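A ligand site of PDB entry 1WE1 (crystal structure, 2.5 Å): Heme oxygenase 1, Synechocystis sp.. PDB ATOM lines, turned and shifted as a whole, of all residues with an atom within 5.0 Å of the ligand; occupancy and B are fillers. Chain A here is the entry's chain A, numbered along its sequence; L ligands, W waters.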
ATOM      1  N   ALA A   6      -7.931  23.251 -35.162  1.00  0.00           N
ATOM      2  CA  ALA A   6      -6.688  23.295 -34.393  1.00  0.00           C
ATOM      3  C   ALA A   6      -5.910  24.580 -34.634  1.00  0.00           C
ATOM      4  O   ALA A   6      -5.437  25.223 -33.687  1.00  0.00           O
ATOM      5  CB  ALA A   6      -5.831  22.077 -34.739  1.00  0.00           C
ATOM      6  N   LEU A   9      -8.191  27.785 -33.676  1.00  0.00           N
ATOM      7  CA  LEU A   9      -8.204  28.110 -32.251  1.00  0.00           C
ATOM      8  C   LEU A   9      -6.880  28.750 -31.884  1.00  0.00           C
ATOM      9  O   LEU A   9      -6.850  29.789 -31.232  1.00  0.00           O
ATOM     10  CB  LEU A   9      -8.439  26.853 -31.400  1.00  0.00           C
ATOM     11  CG  LEU A   9      -9.916  26.486 -31.269  1.00  0.00           C
ATOM     12  CD1 LEU A   9     -10.054  25.098 -30.684  1.00  0.00           C
ATOM     13  CD2 LEU A   9     -10.626  27.506 -30.418  1.00  0.00           C
ATOM     14  N   ARG A  10      -5.783  28.151 -32.337  1.00  0.00           N
ATOM     15  CA  ARG A  10      -4.465  28.685 -32.022  1.00  0.00           C
ATOM     16  C   ARG A  10      -4.284  30.123 -32.509  1.00  0.00           C
ATOM     17  O   ARG A  10      -3.853  30.994 -31.753  1.00  0.00           O
ATOM     18  CB  ARG A  10      -3.354  27.801 -32.605  1.00  0.00           C
ATOM     19  CG  ARG A  10      -1.949  28.312 -32.259  1.00  0.00           C
ATOM     20  CD  ARG A  10      -0.851  27.380 -32.731  1.00  0.00           C
ATOM     21  NE  ARG A  10       0.474  27.993 -32.607  1.00  0.00           N
ATOM     22  CZ  ARG A  10       1.128  28.163 -31.465  1.00  0.00           C
ATOM     23  NH1 ARG A  10       0.591  27.769 -30.316  1.00  0.00           N
ATOM     24  NH2 ARG A  10       2.334  28.736 -31.458  1.00  0.00           N
ATOM     25  N   HIS A  17      -4.532  35.175 -25.198  1.00  0.00           N
ATOM     26  CA  HIS A  17      -3.445  34.575 -24.415  1.00  0.00           C
ATOM     27  C   HIS A  17      -2.450  35.650 -24.029  1.00  0.00           C
ATOM     28  O   HIS A  17      -1.866  35.620 -22.944  1.00  0.00           O
ATOM     29  CB  HIS A  17      -2.756  33.488 -25.226  1.00  0.00           C
ATOM     30  CG  HIS A  17      -1.849  32.617 -24.412  1.00  0.00           C
ATOM     31  ND1 HIS A  17      -0.615  33.041 -23.977  1.00  0.00           N
ATOM     32  CD2 HIS A  17      -1.971  31.329 -23.999  1.00  0.00           C
ATOM     33  CE1 HIS A  17      -0.011  32.054 -23.342  1.00  0.00           C
ATOM     34  NE2 HIS A  17      -0.812  31.003 -23.341  1.00  0.00           N
ATOM     35  N   ALA A  20      -3.756  37.571 -21.194  1.00  0.00           N
ATOM     36  CA  ALA A  20      -3.657  36.720 -20.016  1.00  0.00           C
ATOM     37  C   ALA A  20      -2.307  36.904 -19.334  1.00  0.00           C
ATOM     38  O   ALA A  20      -2.224  37.087 -18.115  1.00  0.00           O
ATOM     39  CB  ALA A  20      -3.857  35.269 -20.433  1.00  0.00           C
ATOM     40  N   GLU A  21      -1.243  36.868 -20.126  1.00  0.00           N
ATOM     41  CA  GLU A  21       0.117  37.020 -19.603  1.00  0.00           C
ATOM     42  C   GLU A  21       0.348  38.384 -18.975  1.00  0.00           C
ATOM     43  O   GLU A  21       1.232  38.533 -18.132  1.00  0.00           O
ATOM     44  CB  GLU A  21       1.133  36.816 -20.724  1.00  0.00           C
ATOM     45  CG  GLU A  21       1.147  35.442 -21.367  1.00  0.00           C
ATOM     46  CD  GLU A  21       1.845  35.475 -22.726  1.00  0.00           C
ATOM     47  OE1 GLU A  21       2.979  36.003 -22.792  1.00  0.00           O
ATOM     48  OE2 GLU A  21       1.263  34.983 -23.711  1.00  0.00           O
ATOM     49  N   VAL A  26      -0.786  37.753 -12.864  1.00  0.00           N
ATOM     50  CA  VAL A  26       0.069  36.902 -13.693  1.00  0.00           C
ATOM     51  C   VAL A  26       1.467  37.469 -13.855  1.00  0.00           C
ATOM     52  O   VAL A  26       2.460  36.734 -13.734  1.00  0.00           O
ATOM     53  CB  VAL A  26      -0.549  36.645 -15.089  1.00  0.00           C
ATOM     54  CG1 VAL A  26       0.497  36.055 -16.054  1.00  0.00           C
ATOM     55  CG2 VAL A  26      -1.726  35.686 -14.941  1.00  0.00           C
ATOM     56  N   LEU A  30       4.839  35.415 -12.886  1.00  0.00           N
ATOM     57  CA  LEU A  30       5.936  35.143 -13.793  1.00  0.00           C
ATOM     58  C   LEU A  30       7.263  35.610 -13.230  1.00  0.00           C
ATOM     59  O   LEU A  30       8.246  34.881 -13.286  1.00  0.00           O
ATOM     60  CB  LEU A  30       5.655  35.799 -15.153  1.00  0.00           C
ATOM     61  CG  LEU A  30       5.196  34.850 -16.268  1.00  0.00           C
ATOM     62  CD1 LEU A  30       4.720  33.524 -15.700  1.00  0.00           C
ATOM     63  CD2 LEU A  30       4.086  35.517 -17.069  1.00  0.00           C
ATOM     64  N   TYR A 125     -10.234  22.793 -24.959  1.00  0.00           N
ATOM     65  CA  TYR A 125      -9.070  23.371 -25.592  1.00  0.00           C
ATOM     66  C   TYR A 125      -8.414  24.369 -24.663  1.00  0.00           C
ATOM     67  O   TYR A 125      -7.255  24.194 -24.306  1.00  0.00           O
ATOM     68  CB  TYR A 125      -9.450  24.057 -26.921  1.00  0.00           C
ATOM     69  CG  TYR A 125      -8.352  24.950 -27.482  1.00  0.00           C
ATOM     70  CD1 TYR A 125      -7.176  24.400 -28.015  1.00  0.00           C
ATOM     71  CD2 TYR A 125      -8.458  26.337 -27.416  1.00  0.00           C
ATOM     72  CE1 TYR A 125      -6.126  25.219 -28.451  1.00  0.00           C
ATOM     73  CE2 TYR A 125      -7.413  27.169 -27.848  1.00  0.00           C
ATOM     74  CZ  TYR A 125      -6.268  26.600 -28.359  1.00  0.00           C
ATOM     75  OH  TYR A 125      -5.242  27.424 -28.741  1.00  0.00           O
ATOM     76  N   THR A 126      -9.155  25.382 -24.251  1.00  0.00           N
ATOM     77  CA  THR A 126      -8.621  26.419 -23.369  1.00  0.00           C
ATOM     78  C   THR A 126      -7.894  25.940 -22.114  1.00  0.00           C
ATOM     79  O   THR A 126      -6.861  26.471 -21.765  1.00  0.00           O
ATOM     80  CB  THR A 126      -9.711  27.425 -22.969  1.00  0.00           C
ATOM     81  OG1 THR A 126     -10.232  28.034 -24.156  1.00  0.00           O
ATOM     82  CG2 THR A 126      -9.134  28.509 -22.082  1.00  0.00           C
ATOM     83  N   ARG A 127      -8.418  24.912 -21.445  1.00  0.00           N
ATOM     84  CA  ARG A 127      -7.743  24.402 -20.257  1.00  0.00           C
ATOM     85  C   ARG A 127      -6.689  23.327 -20.561  1.00  0.00           C
ATOM     86  O   ARG A 127      -5.486  23.573 -20.451  1.00  0.00           O
ATOM     87  CB  ARG A 127      -8.769  23.852 -19.246  1.00  0.00           C
ATOM     88  CG  ARG A 127      -9.569  24.933 -18.500  1.00  0.00           C
ATOM     89  CD  ARG A 127      -8.694  26.102 -18.034  1.00  0.00           C
ATOM     90  NE  ARG A 127      -7.511  25.663 -17.292  1.00  0.00           N
ATOM     91  CZ  ARG A 127      -6.613  26.476 -16.750  1.00  0.00           C
ATOM     92  NH1 ARG A 127      -6.727  27.797 -16.860  1.00  0.00           N
ATOM     93  NH2 ARG A 127      -5.580  25.970 -16.080  1.00  0.00           N
ATOM     94  N   LEU A 129      -5.326  21.915 -23.383  1.00  0.00           N
ATOM     95  CA  LEU A 129      -4.195  22.149 -24.292  1.00  0.00           C
ATOM     96  C   LEU A 129      -3.247  23.206 -23.735  1.00  0.00           C
ATOM     97  O   LEU A 129      -2.071  23.240 -24.088  1.00  0.00           O
ATOM     98  CB  LEU A 129      -4.676  22.523 -25.710  1.00  0.00           C
ATOM     99  CG  LEU A 129      -3.580  22.484 -26.803  1.00  0.00           C
ATOM    100  CD1 LEU A 129      -2.707  21.248 -26.626  1.00  0.00           C
ATOM    101  CD2 LEU A 129      -4.208  22.485 -28.201  1.00  0.00           C
ATOM    102  N   GLY A 130      -3.760  24.054 -22.851  1.00  0.00           N
ATOM    103  CA  GLY A 130      -2.917  25.069 -22.241  1.00  0.00           C
ATOM    104  C   GLY A 130      -2.122  24.444 -21.093  1.00  0.00           C
ATOM    105  O   GLY A 130      -0.936  24.744 -20.923  1.00  0.00           O
ATOM    106  N   SER A 133       0.682  22.527 -22.569  1.00  0.00           N
ATOM    107  CA  SER A 133       1.764  23.317 -23.148  1.00  0.00           C
ATOM    108  C   SER A 133       2.557  24.189 -22.174  1.00  0.00           C
ATOM    109  O   SER A 133       3.760  24.369 -22.356  1.00  0.00           O
ATOM    110  CB  SER A 133       1.219  24.195 -24.262  1.00  0.00           C
ATOM    111  OG  SER A 133       0.470  23.428 -25.186  1.00  0.00           O
ATOM    112  N   GLY A 134       1.871  24.753 -21.182  1.00  0.00           N
ATOM    113  CA  GLY A 134       2.538  25.601 -20.214  1.00  0.00           C
ATOM    114  C   GLY A 134       2.853  24.924 -18.896  1.00  0.00           C
ATOM    115  O   GLY A 134       3.655  25.422 -18.106  1.00  0.00           O
ATOM    116  N   ILE A 137       6.521  25.069 -17.453  1.00  0.00           N
ATOM    117  CA  ILE A 137       7.035  26.380 -17.081  1.00  0.00           C
ATOM    118  C   ILE A 137       6.412  26.854 -15.779  1.00  0.00           C
ATOM    119  O   ILE A 137       7.115  27.228 -14.847  1.00  0.00           O
ATOM    120  CB  ILE A 137       6.727  27.441 -18.156  1.00  0.00           C
ATOM    121  CG1 ILE A 137       7.412  27.052 -19.474  1.00  0.00           C
ATOM    122  CG2 ILE A 137       7.210  28.802 -17.682  1.00  0.00           C
ATOM    123  CD1 ILE A 137       7.213  28.047 -20.609  1.00  0.00           C
ATOM    124  N   LEU A 138       5.084  26.800 -15.727  1.00  0.00           N
ATOM    125  CA  LEU A 138       4.334  27.222 -14.541  1.00  0.00           C
ATOM    126  C   LEU A 138       4.723  26.454 -13.266  1.00  0.00           C
ATOM    127  O   LEU A 138       4.752  27.019 -12.168  1.00  0.00           O
ATOM    128  CB  LEU A 138       2.827  27.071 -14.800  1.00  0.00           C
ATOM    129  CG  LEU A 138       2.338  27.909 -15.993  1.00  0.00           C
ATOM    130  CD1 LEU A 138       0.925  27.496 -16.382  1.00  0.00           C
ATOM    131  CD2 LEU A 138       2.426  29.390 -15.635  1.00  0.00           C
ATOM    132  N   LYS A 168       0.019  15.826 -27.463  1.00  0.00           N
ATOM    133  CA  LYS A 168      -0.392  17.129 -27.932  1.00  0.00           C
ATOM    134  C   LYS A 168      -0.741  17.081 -29.427  1.00  0.00           C
ATOM    135  O   LYS A 168      -1.530  17.876 -29.911  1.00  0.00           O
ATOM    136  CB  LYS A 168       0.718  18.164 -27.654  1.00  0.00           C
ATOM    137  CG  LYS A 168       0.262  19.614 -27.692  1.00  0.00           C
ATOM    138  CD  LYS A 168       1.393  20.597 -27.350  1.00  0.00           C
ATOM    139  CE  LYS A 168       0.999  22.032 -27.690  1.00  0.00           C
ATOM    140  NZ  LYS A 168       2.100  23.033 -27.464  1.00  0.00           N
ATOM    141  N   ARG A 172      -4.439  17.717 -31.172  1.00  0.00           N
ATOM    142  CA  ARG A 172      -4.671  18.719 -32.217  1.00  0.00           C
ATOM    143  C   ARG A 172      -5.312  18.005 -33.399  1.00  0.00           C
ATOM    144  O   ARG A 172      -6.257  18.497 -34.017  1.00  0.00           O
ATOM    145  CB  ARG A 172      -3.356  19.329 -32.690  1.00  0.00           C
ATOM    146  CG  ARG A 172      -2.628  20.189 -31.687  1.00  0.00           C
ATOM    147  CD  ARG A 172      -1.208  20.384 -32.170  1.00  0.00           C
ATOM    148  NE  ARG A 172      -0.445  21.353 -31.387  1.00  0.00           N
ATOM    149  CZ  ARG A 172      -0.774  22.634 -31.264  1.00  0.00           C
ATOM    150  NH1 ARG A 172      -0.005  23.429 -30.526  1.00  0.00           N
ATOM    151  NH2 ARG A 172      -1.853  23.118 -31.870  1.00  0.00           N
ATOM    152  N   PHE A 196     -11.101  32.275 -21.952  1.00  0.00           N
ATOM    153  CA  PHE A 196      -9.910  32.987 -21.553  1.00  0.00           C
ATOM    154  C   PHE A 196     -10.296  34.132 -20.624  1.00  0.00           C
ATOM    155  O   PHE A 196      -9.688  34.326 -19.566  1.00  0.00           O
ATOM    156  CB  PHE A 196      -9.164  33.575 -22.756  1.00  0.00           C
ATOM    157  CG  PHE A 196      -8.084  32.701 -23.287  1.00  0.00           C
ATOM    158  CD1 PHE A 196      -8.371  31.602 -24.093  1.00  0.00           C
ATOM    159  CD2 PHE A 196      -6.745  32.983 -22.998  1.00  0.00           C
ATOM    160  CE1 PHE A 196      -7.337  30.815 -24.605  1.00  0.00           C
ATOM    161  CE2 PHE A 196      -5.721  32.188 -23.494  1.00  0.00           C
ATOM    162  CZ  PHE A 196      -6.024  31.099 -24.305  1.00  0.00           C
ATOM    163  N   ASN A 199     -10.982  33.061 -17.158  1.00  0.00           N
ATOM    164  CA  ASN A 199      -9.804  32.699 -16.388  1.00  0.00           C
ATOM    165  C   ASN A 199      -9.208  34.000 -15.886  1.00  0.00           C
ATOM    166  O   ASN A 199      -8.845  34.135 -14.719  1.00  0.00           O
ATOM    167  CB  ASN A 199      -8.796  31.962 -17.263  1.00  0.00           C
ATOM    168  CG  ASN A 199      -9.147  30.513 -17.446  1.00  0.00           C
ATOM    169  OD1 ASN A 199      -8.863  29.698 -16.577  1.00  0.00           O
ATOM    170  ND2 ASN A 199      -9.783  30.186 -18.545  1.00  0.00           N
ATOM    171  N   MET A 200      -9.141  34.971 -16.788  1.00  0.00           N
ATOM    172  CA  MET A 200      -8.579  36.259 -16.463  1.00  0.00           C
ATOM    173  C   MET A 200      -9.347  36.940 -15.340  1.00  0.00           C
ATOM    174  O   MET A 200      -8.755  37.650 -14.528  1.00  0.00           O
ATOM    175  CB  MET A 200      -8.556  37.139 -17.703  1.00  0.00           C
ATOM    176  CG  MET A 200      -7.597  36.634 -18.770  1.00  0.00           C
ATOM    177  SD  MET A 200      -7.136  37.921 -19.959  1.00  0.00           S
ATOM    178  CE  MET A 200      -8.325  37.597 -21.297  1.00  0.00           C
ATOM    179  N   PHE A 203      -8.196  35.625 -11.983  1.00  0.00           N
ATOM    180  CA  PHE A 203      -6.884  36.185 -11.631  1.00  0.00           C
ATOM    181  C   PHE A 203      -7.027  37.583 -11.047  1.00  0.00           C
ATOM    182  O   PHE A 203      -6.417  37.910 -10.031  1.00  0.00           O
ATOM    183  CB  PHE A 203      -5.972  36.280 -12.849  1.00  0.00           C
ATOM    184  CG  PHE A 203      -5.661  34.972 -13.507  1.00  0.00           C
ATOM    185  CD1 PHE A 203      -5.682  33.776 -12.785  1.00  0.00           C
ATOM    186  CD2 PHE A 203      -5.277  34.932 -14.852  1.00  0.00           C
ATOM    187  CE1 PHE A 203      -5.334  32.560 -13.392  1.00  0.00           C
ATOM    188  CE2 PHE A 203      -4.919  33.726 -15.473  1.00  0.00           C
ATOM    189  CZ  PHE A 203      -4.937  32.537 -14.745  1.00  0.00           C
HETATM  190  C1  LIG L   1      -0.084  27.740 -25.058  1.00  0.00           C
HETATM  191  C2  LIG L   1      -4.107  28.395 -22.459  1.00  0.00           C
HETATM  192  C3  LIG L   1      -1.628  31.553 -19.729  1.00  0.00           C
HETATM  193  C4  LIG L   1       2.455  29.643 -21.371  1.00  0.00           C
HETATM  194  C5  LIG L   1      -1.446  27.726 -24.698  1.00  0.00           C
HETATM  195  C6  LIG L   1      -2.534  27.113 -25.453  1.00  0.00           C
HETATM  196  C7  LIG L   1      -3.681  27.340 -24.741  1.00  0.00           C
HETATM  197  C8  LIG L   1      -3.274  28.042 -23.509  1.00  0.00           C
HETATM  198  C9  LIG L   1      -5.094  26.949 -25.077  1.00  0.00           C
HETATM  199  C10 LIG L   1      -2.389  26.309 -26.733  1.00  0.00           C
HETATM  200  C11 LIG L   1      -2.168  27.148 -28.024  1.00  0.00           C
HETATM  201  C12 LIG L   1      -2.057  26.388 -29.208  1.00  0.00           C
HETATM  202  O1  LIG L   1      -3.122  26.342 -29.952  1.00  0.00           O
HETATM  203  O2  LIG L   1      -1.030  25.772 -29.544  1.00  0.00           O
HETATM  204  C13 LIG L   1      -3.794  29.364 -21.484  1.00  0.00           C
HETATM  205  C14 LIG L   1      -4.773  29.986 -20.590  1.00  0.00           C
HETATM  206  C15 LIG L   1      -4.064  30.830 -19.782  1.00  0.00           C
HETATM  207  C16 LIG L   1      -2.687  30.771 -20.241  1.00  0.00           C
HETATM  208  C17 LIG L   1      -6.253  29.686 -20.596  1.00  0.00           C
HETATM  209  C18 LIG L   1      -4.551  31.640 -18.595  1.00  0.00           C
HETATM  210  C19 LIG L   1      -5.575  32.746 -18.948  1.00  0.00           C
HETATM  211  C20 LIG L   1      -0.293  31.255 -19.861  1.00  0.00           C
HETATM  212  C21 LIG L   1       0.784  31.804 -19.043  1.00  0.00           C
HETATM  213  C22 LIG L   1       1.923  31.435 -19.669  1.00  0.00           C
HETATM  214  C23 LIG L   1       1.571  30.441 -20.659  1.00  0.00           C
HETATM  215  C24 LIG L   1       0.590  32.589 -17.767  1.00  0.00           C
HETATM  216  C25 LIG L   1       3.328  31.979 -19.424  1.00  0.00           C
HETATM  217  C26 LIG L   1       4.067  31.133 -18.348  1.00  0.00           C
HETATM  218  C27 LIG L   1       2.139  28.918 -22.541  1.00  0.00           C
HETATM  219  C28 LIG L   1       3.130  28.273 -23.401  1.00  0.00           C
HETATM  220  C29 LIG L   1       2.413  27.701 -24.404  1.00  0.00           C
HETATM  221  C30 LIG L   1       0.992  28.052 -24.192  1.00  0.00           C
HETATM  222  C31 LIG L   1       4.593  28.308 -23.131  1.00  0.00           C
HETATM  223  C32 LIG L   1       2.873  26.860 -25.574  1.00  0.00           C
HETATM  224  C33 LIG L   1       3.093  27.722 -26.892  1.00  0.00           C
HETATM  225  C34 LIG L   1       3.247  26.925 -28.055  1.00  0.00           C
HETATM  226  O3  LIG L   1       2.501  25.894 -28.247  1.00  0.00           O
HETATM  227  O4  LIG L   1       4.127  27.228 -28.919  1.00  0.00           O
HETATM  228  N1  LIG L   1      -1.920  28.305 -23.542  1.00  0.00           N
HETATM  229  N2  LIG L   1      -2.530  29.840 -21.253  1.00  0.00           N
HETATM  230  N3  LIG L   1       0.212  30.376 -20.835  1.00  0.00           N
HETATM  231  N4  LIG L   1       0.841  28.725 -23.032  1.00  0.00           N
HETATM  232 FE1  LIG L   1      -0.839  29.318 -22.185  1.00  0.00          FE
HETATM  233  O   HOH W   1      -0.822  27.808 -21.205  1.00  0.00           O
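An oxygen (O2) of the ligand is in salt-bridge range of the guanidinium group (NH1) of Arg 10 (2.7 Å).
OH of Tyr 125 lies within hydrogen-bond range of O1 of the ligand (2.7 Å).
NE2 of His 17 is bound to FE1 of the ligand (2.0 Å).
NH1 of Arg 172 is in salt-bridge range of O2 of the ligand, at 2.7 Å.
An oxygen (O3) of the ligand lies within salt-bridge range of the side-chain amino group (NZ) of Lys 168.
A ring nitrogen (ND1) of His 17 is in hydrogen-bond range of the side-chain carboxylate of Glu 21 (2.7 Å).
The backbone carbonyl oxygen (O) of Leu 129 is in hydrogen-bond range of the side-chain hydroxyl (OG) of Ser 133 (2.8 Å).
The backbone NH (N) of Ala 20 lies within hydrogen-bond range of the side-chain sulfur (SD) of Met 200.
The side-chain amide oxygen (OD1) of Asn 199 is in hydrogen-bond range of the guanidinium group (NH1) of Arg 127.
The side-chain hydroxyl (OG) of Ser 133 is in hydrogen-bond range of the side-chain amino group (NZ) of Lys 168, 2.8 Å away.
CB of Ala 20 touches C19 of the ligand (3.4 Å).
Val 26 touches the ligand (CG1 to C24, 3.9 Å).
Leu 30 touches the ligand.
O of Thr 126 touches C2 of the ligand, at 3.4 Å.
Gly 130 touches the ligand (CA to C8, 3.3 Å).
Ser 133 touches the ligand.
Ile 137 touches the ligand (CD1 to C31, 3.6 Å).
Leu 138 touches the ligand.
Phe 196 touches the ligand.
Asn 199 touches the ligand.
Phe 203 touches the ligand.
Hydrophobic or aromatic side chains that line the ligand: His 17, Ala 20, Val 26, Leu 30, Tyr 125, Ile 137, Leu 138, Phe 196 and Phe 203.
Of the 23 residues printed, 16 come within 4 Å of the ligand.
The nearest printed residue that does not touch the ligand is Leu 129 (4.01 Å).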
